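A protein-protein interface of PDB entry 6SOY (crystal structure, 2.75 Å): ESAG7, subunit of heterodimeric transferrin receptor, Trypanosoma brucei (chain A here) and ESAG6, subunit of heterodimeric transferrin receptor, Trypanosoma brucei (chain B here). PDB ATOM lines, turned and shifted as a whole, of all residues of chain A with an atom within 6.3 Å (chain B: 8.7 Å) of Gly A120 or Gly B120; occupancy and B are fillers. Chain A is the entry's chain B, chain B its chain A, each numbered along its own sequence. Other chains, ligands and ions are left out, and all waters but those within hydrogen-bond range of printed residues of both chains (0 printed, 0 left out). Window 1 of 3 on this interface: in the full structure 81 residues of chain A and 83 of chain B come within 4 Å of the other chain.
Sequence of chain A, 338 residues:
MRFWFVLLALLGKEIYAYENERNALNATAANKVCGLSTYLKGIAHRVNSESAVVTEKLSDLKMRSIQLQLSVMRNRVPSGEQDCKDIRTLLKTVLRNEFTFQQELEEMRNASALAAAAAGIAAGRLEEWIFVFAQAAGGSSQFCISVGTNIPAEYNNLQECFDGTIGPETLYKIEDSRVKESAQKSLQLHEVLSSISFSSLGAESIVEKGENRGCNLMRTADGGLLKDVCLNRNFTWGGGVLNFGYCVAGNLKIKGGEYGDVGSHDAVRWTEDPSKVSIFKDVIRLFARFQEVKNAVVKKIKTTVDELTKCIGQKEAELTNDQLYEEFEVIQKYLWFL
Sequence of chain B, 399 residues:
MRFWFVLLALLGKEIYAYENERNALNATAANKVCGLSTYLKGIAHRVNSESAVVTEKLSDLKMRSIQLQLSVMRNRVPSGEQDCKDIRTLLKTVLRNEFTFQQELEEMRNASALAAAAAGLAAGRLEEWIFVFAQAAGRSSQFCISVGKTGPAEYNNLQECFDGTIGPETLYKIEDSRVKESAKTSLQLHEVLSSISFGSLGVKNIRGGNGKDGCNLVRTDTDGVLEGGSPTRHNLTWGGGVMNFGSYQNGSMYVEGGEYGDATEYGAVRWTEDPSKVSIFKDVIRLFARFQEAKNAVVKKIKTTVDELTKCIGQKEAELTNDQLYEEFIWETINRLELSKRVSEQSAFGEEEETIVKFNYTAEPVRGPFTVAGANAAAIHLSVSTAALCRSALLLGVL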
ATOM      1  N   LEU A  40     -26.452  11.978  14.354  1.00  0.00           N
ATOM      2  CA  LEU A  40     -25.570  11.355  15.340  1.00  0.00           C
ATOM      3  C   LEU A  40     -25.620   9.833  15.303  1.00  0.00           C
ATOM      4  O   LEU A  40     -24.620   9.188  15.584  1.00  0.00           O
ATOM      5  CB  LEU A  40     -25.839  11.901  16.757  1.00  0.00           C
ATOM      6  CG  LEU A  40     -25.579  13.412  17.020  1.00  0.00           C
ATOM      7  CD1 LEU A  40     -26.435  13.909  18.153  1.00  0.00           C
ATOM      8  CD2 LEU A  40     -24.081  13.730  17.303  1.00  0.00           C
ATOM      9  N   LYS A  41     -26.767   9.253  14.945  1.00  0.00           N
ATOM     10  CA  LYS A  41     -26.928   7.801  14.796  1.00  0.00           C
ATOM     11  C   LYS A  41     -26.138   7.359  13.551  1.00  0.00           C
ATOM     12  O   LYS A  41     -25.565   6.277  13.528  1.00  0.00           O
ATOM     13  CB  LYS A  41     -28.409   7.458  14.586  1.00  0.00           C
ATOM     14  CG  LYS A  41     -29.279   7.667  15.798  1.00  0.00           C
ATOM     15  CD  LYS A  41     -30.712   7.633  15.369  1.00  0.00           C
ATOM     16  CE  LYS A  41     -31.658   7.756  16.530  1.00  0.00           C
ATOM     17  NZ  LYS A  41     -33.007   8.153  16.058  1.00  0.00           N
ATOM     18  N   ALA A 115     -16.217   7.041  18.993  1.00  0.00           N
ATOM     19  CA  ALA A 115     -16.894   8.156  18.334  1.00  0.00           C
ATOM     20  C   ALA A 115     -18.318   7.734  17.959  1.00  0.00           C
ATOM     21  O   ALA A 115     -19.242   8.488  18.223  1.00  0.00           O
ATOM     22  CB  ALA A 115     -16.114   8.602  17.113  1.00  0.00           C
ATOM     23  N   ALA A 116     -18.508   6.484  17.461  1.00  0.00           N
ATOM     24  CA  ALA A 116     -19.826   5.937  17.140  1.00  0.00           C
ATOM     25  C   ALA A 116     -20.728   5.754  18.392  1.00  0.00           C
ATOM     26  O   ALA A 116     -21.907   6.056  18.313  1.00  0.00           O
ATOM     27  CB  ALA A 116     -19.678   4.636  16.385  1.00  0.00           C
ATOM     28  N   ALA A 117     -20.168   5.301  19.534  1.00  0.00           N
ATOM     29  CA  ALA A 117     -20.847   5.087  20.832  1.00  0.00           C
ATOM     30  C   ALA A 117     -21.239   6.413  21.519  1.00  0.00           C
ATOM     31  O   ALA A 117     -22.414   6.602  21.864  1.00  0.00           O
ATOM     32  CB  ALA A 117     -19.953   4.274  21.757  1.00  0.00           C
ATOM     33  N   ALA A 118     -20.241   7.328  21.705  1.00  0.00           N
ATOM     34  CA  ALA A 118     -20.390   8.673  22.273  1.00  0.00           C
ATOM     35  C   ALA A 118     -21.456   9.475  21.515  1.00  0.00           C
ATOM     36  O   ALA A 118     -22.206  10.232  22.140  1.00  0.00           O
ATOM     37  CB  ALA A 118     -19.062   9.406  22.221  1.00  0.00           C
ATOM     38  N   ALA A 119     -21.526   9.285  20.171  1.00  0.00           N
ATOM     39  CA  ALA A 119     -22.506   9.930  19.301  1.00  0.00           C
ATOM     40  C   ALA A 119     -23.886   9.354  19.614  1.00  0.00           C
ATOM     41  O   ALA A 119     -24.806  10.138  19.878  1.00  0.00           O
ATOM     42  CB  ALA A 119     -22.150   9.712  17.840  1.00  0.00           C
ATOM     43  N   GLY A 120     -23.990   8.009  19.668  1.00  0.00           N
ATOM     44  CA  GLY A 120     -25.193   7.274  20.058  1.00  0.00           C
ATOM     45  C   GLY A 120     -25.695   7.680  21.439  1.00  0.00           C
ATOM     46  O   GLY A 120     -26.906   7.748  21.649  1.00  0.00           O
ATOM     47  N   ILE A 121     -24.793   8.011  22.395  1.00  0.00           N
ATOM     48  CA  ILE A 121     -25.285   8.506  23.698  1.00  0.00           C
ATOM     49  C   ILE A 121     -26.040   9.826  23.482  1.00  0.00           C
ATOM     50  O   ILE A 121     -27.216   9.914  23.835  1.00  0.00           O
ATOM     51  CB  ILE A 121     -24.254   8.596  24.871  1.00  0.00           C
ATOM     52  CG1 ILE A 121     -23.491   7.278  25.069  1.00  0.00           C
ATOM     53  CG2 ILE A 121     -24.959   8.989  26.162  1.00  0.00           C
ATOM     54  CD1 ILE A 121     -22.075   7.439  25.540  1.00  0.00           C
ATOM     55  N   ALA A 122     -25.404  10.801  22.809  1.00  0.00           N
ATOM     56  CA  ALA A 122     -26.019  12.089  22.530  1.00  0.00           C
ATOM     57  C   ALA A 122     -27.332  11.931  21.766  1.00  0.00           C
ATOM     58  O   ALA A 122     -28.255  12.694  22.017  1.00  0.00           O
ATOM     59  CB  ALA A 122     -25.060  12.975  21.758  1.00  0.00           C
ATOM     60  N   ALA A 123     -27.434  10.944  20.862  1.00  0.00           N
ATOM     61  CA  ALA A 123     -28.657  10.680  20.099  1.00  0.00           C
ATOM     62  C   ALA A 123     -29.813  10.223  21.013  1.00  0.00           C
ATOM     63  O   ALA A 123     -30.932  10.688  20.848  1.00  0.00           O
ATOM     64  CB  ALA A 123     -28.387   9.625  19.042  1.00  0.00           C
ATOM     65  N   GLY A 124     -29.519   9.349  21.977  1.00  0.00           N
ATOM     66  CA  GLY A 124     -30.501   8.789  22.891  1.00  0.00           C
ATOM     67  C   GLY A 124     -31.022   9.794  23.883  1.00  0.00           C
ATOM     68  O   GLY A 124     -32.215   9.777  24.235  1.00  0.00           O
ATOM     69  N   ARG A 125     -30.112  10.677  24.339  1.00  0.00           N
ATOM     70  CA  ARG A 125     -30.424  11.725  25.304  1.00  0.00           C
ATOM     71  C   ARG A 125     -31.436  12.678  24.722  1.00  0.00           C
ATOM     72  O   ARG A 125     -32.464  12.919  25.349  1.00  0.00           O
ATOM     73  CB  ARG A 125     -29.154  12.419  25.796  1.00  0.00           C
ATOM     74  CG  ARG A 125     -28.445  11.606  26.891  1.00  0.00           C
ATOM     75  CD  ARG A 125     -28.848  12.029  28.309  1.00  0.00           C
ATOM     76  NE  ARG A 125     -27.673  12.476  29.056  1.00  0.00           N
ATOM     77  CZ  ARG A 125     -27.565  13.638  29.688  1.00  0.00           C
ATOM     78  NH1 ARG A 125     -28.587  14.479  29.726  1.00  0.00           N
ATOM     79  NH2 ARG A 125     -26.427  13.968  30.294  1.00  0.00           N
ATOM     80  N   VAL A 283     -18.588  13.938  21.526  1.00  0.00           N
ATOM     81  CA  VAL A 283     -18.811  13.567  20.124  1.00  0.00           C
ATOM     82  C   VAL A 283     -17.774  14.311  19.257  1.00  0.00           C
ATOM     83  O   VAL A 283     -17.192  13.713  18.349  1.00  0.00           O
ATOM     84  CB  VAL A 283     -20.252  13.825  19.620  1.00  0.00           C
ATOM     85  CG1 VAL A 283     -20.491  13.048  18.338  1.00  0.00           C
ATOM     86  CG2 VAL A 283     -21.301  13.469  20.667  1.00  0.00           C
ATOM     87  N   SER B  37     -26.969   1.140  31.994  1.00  0.00           N
ATOM     88  CA  SER B  37     -26.516   2.199  31.092  1.00  0.00           C
ATOM     89  C   SER B  37     -24.980   2.302  31.008  1.00  0.00           C
ATOM     90  O   SER B  37     -24.475   2.519  29.917  1.00  0.00           O
ATOM     91  CB  SER B  37     -27.097   3.531  31.526  1.00  0.00           C
ATOM     92  OG  SER B  37     -26.793   4.540  30.582  1.00  0.00           O
ATOM     93  N   TYR B  39     -22.967  -0.169  31.521  1.00  0.00           N
ATOM     94  CA  TYR B  39     -22.549  -1.426  30.886  1.00  0.00           C
ATOM     95  C   TYR B  39     -22.638  -1.232  29.385  1.00  0.00           C
ATOM     96  O   TYR B  39     -21.712  -1.614  28.671  1.00  0.00           O
ATOM     97  CB  TYR B  39     -23.391  -2.637  31.349  1.00  0.00           C
ATOM     98  CG  TYR B  39     -22.914  -3.957  30.771  1.00  0.00           C
ATOM     99  CD1 TYR B  39     -23.260  -4.340  29.474  1.00  0.00           C
ATOM    100  CD2 TYR B  39     -22.107  -4.821  31.516  1.00  0.00           C
ATOM    101  CE1 TYR B  39     -22.826  -5.550  28.937  1.00  0.00           C
ATOM    102  CE2 TYR B  39     -21.683  -6.046  30.992  1.00  0.00           C
ATOM    103  CZ  TYR B  39     -22.052  -6.407  29.701  1.00  0.00           C
ATOM    104  OH  TYR B  39     -21.615  -7.573  29.123  1.00  0.00           O
ATOM    105  N   LEU B  40     -23.725  -0.577  28.929  1.00  0.00           N
ATOM    106  CA  LEU B  40     -24.004  -0.274  27.524  1.00  0.00           C
ATOM    107  C   LEU B  40     -22.994   0.696  26.954  1.00  0.00           C
ATOM    108  O   LEU B  40     -22.549   0.458  25.850  1.00  0.00           O
ATOM    109  CB  LEU B  40     -25.465   0.175  27.305  1.00  0.00           C
ATOM    110  CG  LEU B  40     -26.506  -0.910  27.586  1.00  0.00           C
ATOM    111  CD1 LEU B  40     -27.857  -0.329  27.879  1.00  0.00           C
ATOM    112  CD2 LEU B  40     -26.557  -1.930  26.482  1.00  0.00           C
ATOM    113  N   LYS B  41     -22.534   1.707  27.725  1.00  0.00           N
ATOM    114  CA  LYS B  41     -21.439   2.623  27.318  1.00  0.00           C
ATOM    115  C   LYS B  41     -20.120   1.847  27.190  1.00  0.00           C
ATOM    116  O   LYS B  41     -19.326   2.142  26.307  1.00  0.00           O
ATOM    117  CB  LYS B  41     -21.243   3.750  28.335  1.00  0.00           C
ATOM    118  CG  LYS B  41     -22.271   4.856  28.277  1.00  0.00           C
ATOM    119  CD  LYS B  41     -22.256   5.637  29.558  1.00  0.00           C
ATOM    120  CE  LYS B  41     -23.587   6.290  29.787  1.00  0.00           C
ATOM    121  NZ  LYS B  41     -23.545   7.246  30.920  1.00  0.00           N
ATOM    122  N   GLY B  42     -19.928   0.840  28.036  1.00  0.00           N
ATOM    123  CA  GLY B  42     -18.751  -0.027  28.026  1.00  0.00           C
ATOM    124  C   GLY B  42     -18.654  -1.006  26.867  1.00  0.00           C
ATOM    125  O   GLY B  42     -17.570  -1.546  26.624  1.00  0.00           O
ATOM    126  N   ILE B  43     -19.786  -1.251  26.141  1.00  0.00           N
ATOM    127  CA  ILE B  43     -19.867  -2.153  24.981  1.00  0.00           C
ATOM    128  C   ILE B  43     -18.870  -1.722  23.898  1.00  0.00           C
ATOM    129  O   ILE B  43     -18.284  -2.584  23.230  1.00  0.00           O
ATOM    130  CB  ILE B  43     -21.316  -2.330  24.472  1.00  0.00           C
ATOM    131  CG1 ILE B  43     -22.047  -3.352  25.363  1.00  0.00           C
ATOM    132  CG2 ILE B  43     -21.353  -2.747  22.996  1.00  0.00           C
ATOM    133  CD1 ILE B  43     -23.488  -3.605  25.061  1.00  0.00           C
ATOM    134  N   ALA B  44     -18.630  -0.395  23.789  1.00  0.00           N
ATOM    135  CA  ALA B  44     -17.656   0.235  22.897  1.00  0.00           C
ATOM    136  C   ALA B  44     -16.263  -0.326  23.199  1.00  0.00           C
ATOM    137  O   ALA B  44     -15.543  -0.694  22.279  1.00  0.00           O
ATOM    138  CB  ALA B  44     -17.654   1.732  23.139  1.00  0.00           C
ATOM    139  N   ALA B 113     -18.615  -1.185  15.321  1.00  0.00           N
ATOM    140  CA  ALA B 113     -19.016   0.231  15.428  1.00  0.00           C
ATOM    141  C   ALA B 113     -20.524   0.402  15.540  1.00  0.00           C
ATOM    142  O   ALA B 113     -20.962   1.325  16.233  1.00  0.00           O
ATOM    143  CB  ALA B 113     -18.488   1.038  14.255  1.00  0.00           C
ATOM    144  N   LEU B 114     -21.311  -0.470  14.854  1.00  0.00           N
ATOM    145  CA  LEU B 114     -22.784  -0.461  14.878  1.00  0.00           C
ATOM    146  C   LEU B 114     -23.267  -0.940  16.258  1.00  0.00           C
ATOM    147  O   LEU B 114     -24.107  -0.278  16.847  1.00  0.00           O
ATOM    148  CB  LEU B 114     -23.406  -1.289  13.719  1.00  0.00           C
ATOM    149  CG  LEU B 114     -23.026  -0.901  12.244  1.00  0.00           C
ATOM    150  CD1 LEU B 114     -23.496  -1.919  11.284  1.00  0.00           C
ATOM    151  CD2 LEU B 114     -23.571   0.452  11.814  1.00  0.00           C
ATOM    152  N   ALA B 115     -22.667  -2.023  16.812  1.00  0.00           N
ATOM    153  CA  ALA B 115     -22.928  -2.528  18.173  1.00  0.00           C
ATOM    154  C   ALA B 115     -22.625  -1.412  19.223  1.00  0.00           C
ATOM    155  O   ALA B 115     -23.438  -1.183  20.125  1.00  0.00           O
ATOM    156  CB  ALA B 115     -22.066  -3.748  18.451  1.00  0.00           C
ATOM    157  N   ALA B 116     -21.486  -0.686  19.053  1.00  0.00           N
ATOM    158  CA  ALA B 116     -21.064   0.442  19.887  1.00  0.00           C
ATOM    159  C   ALA B 116     -22.137   1.555  19.907  1.00  0.00           C
ATOM    160  O   ALA B 116     -22.578   1.968  20.983  1.00  0.00           O
ATOM    161  CB  ALA B 116     -19.748   1.003  19.371  1.00  0.00           C
ATOM    162  N   ALA B 117     -22.566   2.009  18.716  1.00  0.00           N
ATOM    163  CA  ALA B 117     -23.556   3.065  18.547  1.00  0.00           C
ATOM    164  C   ALA B 117     -24.902   2.696  19.116  1.00  0.00           C
ATOM    165  O   ALA B 117     -25.440   3.480  19.908  1.00  0.00           O
ATOM    166  CB  ALA B 117     -23.689   3.441  17.084  1.00  0.00           C
ATOM    167  N   ALA B 118     -25.438   1.507  18.743  1.00  0.00           N
ATOM    168  CA  ALA B 118     -26.730   0.995  19.197  1.00  0.00           C
ATOM    169  C   ALA B 118     -26.799   0.945  20.736  1.00  0.00           C
ATOM    170  O   ALA B 118     -27.818   1.345  21.305  1.00  0.00           O
ATOM    171  CB  ALA B 118     -26.994  -0.379  18.601  1.00  0.00           C
ATOM    172  N   ALA B 119     -25.718   0.462  21.404  1.00  0.00           N
ATOM    173  CA  ALA B 119     -25.610   0.403  22.862  1.00  0.00           C
ATOM    174  C   ALA B 119     -25.503   1.811  23.457  1.00  0.00           C
ATOM    175  O   ALA B 119     -26.104   2.080  24.502  1.00  0.00           O
ATOM    176  CB  ALA B 119     -24.411  -0.415  23.255  1.00  0.00           C
ATOM    177  N   GLY B 120     -24.754   2.701  22.788  1.00  0.00           N
ATOM    178  CA  GLY B 120     -24.640   4.111  23.160  1.00  0.00           C
ATOM    179  C   GLY B 120     -26.015   4.772  23.194  1.00  0.00           C
ATOM    180  O   GLY B 120     -26.324   5.471  24.160  1.00  0.00           O
ATOM    181  N   LEU B 121     -26.888   4.469  22.182  1.00  0.00           N
ATOM    182  CA  LEU B 121     -28.281   4.945  22.075  1.00  0.00           C
ATOM    183  C   LEU B 121     -29.120   4.531  23.290  1.00  0.00           C
ATOM    184  O   LEU B 121     -29.681   5.397  23.968  1.00  0.00           O
ATOM    185  CB  LEU B 121     -28.955   4.371  20.818  1.00  0.00           C
ATOM    186  CG  LEU B 121     -29.669   5.311  19.858  1.00  0.00           C
ATOM    187  CD1 LEU B 121     -30.222   4.530  18.689  1.00  0.00           C
ATOM    188  CD2 LEU B 121     -30.786   6.089  20.513  1.00  0.00           C
ATOM    189  N   ALA B 122     -29.235   3.194  23.527  1.00  0.00           N
ATOM    190  CA  ALA B 122     -29.983   2.598  24.629  1.00  0.00           C
ATOM    191  C   ALA B 122     -29.564   3.255  25.958  1.00  0.00           C
ATOM    192  O   ALA B 122     -30.432   3.632  26.740  1.00  0.00           O
ATOM    193  CB  ALA B 122     -29.758   1.088  24.665  1.00  0.00           C
ATOM    194  N   ALA B 123     -28.251   3.486  26.152  1.00  0.00           N
ATOM    195  CA  ALA B 123     -27.696   4.154  27.334  1.00  0.00           C
ATOM    196  C   ALA B 123     -28.147   5.638  27.475  1.00  0.00           C
ATOM    197  O   ALA B 123     -28.458   6.067  28.579  1.00  0.00           O
ATOM    198  CB  ALA B 123     -26.175   4.049  27.327  1.00  0.00           C
ATOM    199  N   GLY B 124     -28.189   6.379  26.365  1.00  0.00           N
ATOM    200  CA  GLY B 124     -28.596   7.780  26.343  1.00  0.00           C
ATOM    201  C   GLY B 124     -30.040   7.969  26.758  1.00  0.00           C
ATOM    202  O   GLY B 124     -30.383   8.893  27.504  1.00  0.00           O
ATOM    203  N   ARG B 125     -30.880   7.035  26.310  1.00  0.00           N
ATOM    204  CA  ARG B 125     -32.317   6.928  26.547  1.00  0.00           C
ATOM    205  C   ARG B 125     -32.563   6.707  28.004  1.00  0.00           C
ATOM    206  O   ARG B 125     -33.271   7.503  28.608  1.00  0.00           O
ATOM    207  CB  ARG B 125     -32.897   5.777  25.702  1.00  0.00           C
ATOM    208  CG  ARG B 125     -32.848   6.047  24.186  1.00  0.00           C
ATOM    209  CD  ARG B 125     -33.990   6.955  23.700  1.00  0.00           C
ATOM    210  NE  ARG B 125     -34.884   6.217  22.807  1.00  0.00           N
ATOM    211  CZ  ARG B 125     -36.071   5.755  23.163  1.00  0.00           C
ATOM    212  NH1 ARG B 125     -36.544   5.999  24.370  1.00  0.00           N
ATOM    213  NH2 ARG B 125     -36.807   5.058  22.303  1.00  0.00           N
ATOM    214  N   LEU B 126     -31.917   5.677  28.596  1.00  0.00           N
ATOM    215  CA  LEU B 126     -32.024   5.325  30.006  1.00  0.00           C
ATOM    216  C   LEU B 126     -31.476   6.462  30.851  1.00  0.00           C
ATOM    217  O   LEU B 126     -32.134   6.854  31.805  1.00  0.00           O
ATOM    218  CB  LEU B 126     -31.233   4.031  30.308  1.00  0.00           C
ATOM    219  CG  LEU B 126     -31.660   2.690  29.674  1.00  0.00           C
ATOM    220  CD1 LEU B 126     -30.713   1.605  30.095  1.00  0.00           C
ATOM    221  CD2 LEU B 126     -33.119   2.294  30.049  1.00  0.00           C
ATOM    222  N   GLU B 127     -30.287   7.011  30.510  1.00  0.00           N
ATOM    223  CA  GLU B 127     -29.665   8.127  31.251  1.00  0.00           C
ATOM    224  C   GLU B 127     -30.553   9.369  31.248  1.00  0.00           C
ATOM    225  O   GLU B 127     -30.639  10.017  32.287  1.00  0.00           O
ATOM    226  CB  GLU B 127     -28.272   8.471  30.700  1.00  0.00           C
ATOM    227  CG  GLU B 127     -27.510   9.523  31.491  1.00  0.00           C
ATOM    228  CD  GLU B 127     -26.001   9.424  31.388  1.00  0.00           C
ATOM    229  OE1 GLU B 127     -25.456   9.736  30.306  1.00  0.00           O
ATOM    230  OE2 GLU B 127     -25.362   9.044  32.399  1.00  0.00           O
ATOM    231  N   ILE B 174     -18.298   8.184  28.522  1.00  0.00           N
ATOM    232  CA  ILE B 174     -17.739   6.955  27.931  1.00  0.00           C
ATOM    233  C   ILE B 174     -16.282   6.636  28.353  1.00  0.00           C
ATOM    234  O   ILE B 174     -15.967   5.450  28.489  1.00  0.00           O
ATOM    235  CB  ILE B 174     -17.912   6.954  26.368  1.00  0.00           C
ATOM    236  CG1 ILE B 174     -17.853   5.545  25.782  1.00  0.00           C
ATOM    237  CG2 ILE B 174     -16.961   7.896  25.634  1.00  0.00           C
ATOM    238  CD1 ILE B 174     -19.016   5.208  25.146  1.00  0.00           C
ATOM    239  N   ILE B 280     -35.158  -0.653  22.436  1.00  0.00           N
ATOM    240  CA  ILE B 280     -33.779  -0.209  22.427  1.00  0.00           C
ATOM    241  C   ILE B 280     -32.797  -1.361  22.694  1.00  0.00           C
ATOM    242  O   ILE B 280     -31.692  -1.326  22.146  1.00  0.00           O
ATOM    243  CB  ILE B 280     -33.552   1.036  23.346  1.00  0.00           C
ATOM    244  CG1 ILE B 280     -34.204   0.888  24.741  1.00  0.00           C
ATOM    245  CG2 ILE B 280     -34.057   2.314  22.657  1.00  0.00           C
ATOM    246  CD1 ILE B 280     -33.831   2.009  25.782  1.00  0.00           C
ATOM    247  N   VAL B 284     -29.410  -3.923  20.362  1.00  0.00           N
ATOM    248  CA  VAL B 284     -28.116  -4.114  21.009  1.00  0.00           C
ATOM    249  C   VAL B 284     -27.801  -5.610  21.004  1.00  0.00           C
ATOM    250  O   VAL B 284     -26.727  -6.011  20.537  1.00  0.00           O
ATOM    251  CB  VAL B 284     -28.042  -3.444  22.404  1.00  0.00           C
ATOM    252  CG1 VAL B 284     -26.656  -3.609  23.015  1.00  0.00           C
ATOM    253  CG2 VAL B 284     -28.401  -1.962  22.304  1.00  0.00           C
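O of Gly A120 sits close to N of Leu B121 (3.3 Å).
O of Gly A120 sits close to O of Gly B120 (3.4 Å).
The side-chain carboxylate (OE1) of Glu B127 lies within salt-bridge range of the guanidinium group (NE) of Arg A125.
N of Ile A121 sits close to O of Gly B120, at 3.5 Å.
The side-chain amino group of Lys B41 is in salt-bridge range of the side-chain carboxylate of Glu B127, 3.0 Å away.
Among the printed residues, pairs that only touch across the chains: Ala A116 with Ala B113, Ala A116 with Ala B117, Ala A117 with Ala B44, Ala A117 with Ala B116, Ala A117 with Gly B120, Ala A117 with Ile B174, Gly A120 with Ala B117, Ile A121 with Lys B41, Ile A121 with Gly B124, Ile A121 with Ile B174, Gly A124 with Leu B121, Gly A124 with Gly B124, Gly A124 with Arg B125 and Arg A125 with Gly B124.
Of the printed residues of chain B, Gly A120 touches Ala B117, Gly B120 and Leu B121.
Gly B120 touches just these residues of chain A: Ala A117, Gly A120 and Ile A121.
No residue of chain B comes within 4 Å of Ala A119.
Of the printed residues of chain B, Gly A124 touches Leu B121 (3.6 Å), Gly B124 (3.5 Å) and Arg B125 (3.4 Å).
Of the printed residues of chain B, Ile A121 touches Lys B41, Gly B120, Gly B124 and Ile B174.
Printed residues of chain B within 4 Å of Ala A117: Ala B44 (3.7 Å), Ala B116 (3.6 Å), Gly B120 (3.6 Å) and Ile B174 (3.6 Å).
Printed residues of chain A within 4 Å of Ala B117: Ala A116 (3.4 Å) and Gly A120 (3.8 Å).
The nearest printed residue of chain A that does not touch Ala B117 is Ala A117 (4.1 Å).
Of the 14 printed residues of chain A, 6 touch a printed residue of chain B.
Of the 25 printed residues of chain B, 11 touch a printed residue of chain A.
Hydrophobic or aromatic side chains of chain B within 4 Å of the printed part of chain A: Ala B44, Ala B117, Leu B121 and Ile B174.
Along chain B the printed residues that touch a printed residue of chain A span positions 41 to 174.
Among the printed residues, 18 pairs touch across the chains.
Among the printed residues, Asp or Glu carboxylates within 4 Å of a Lys or Arg side-chain nitrogen of the other chain: Arg A125 with Glu B127.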
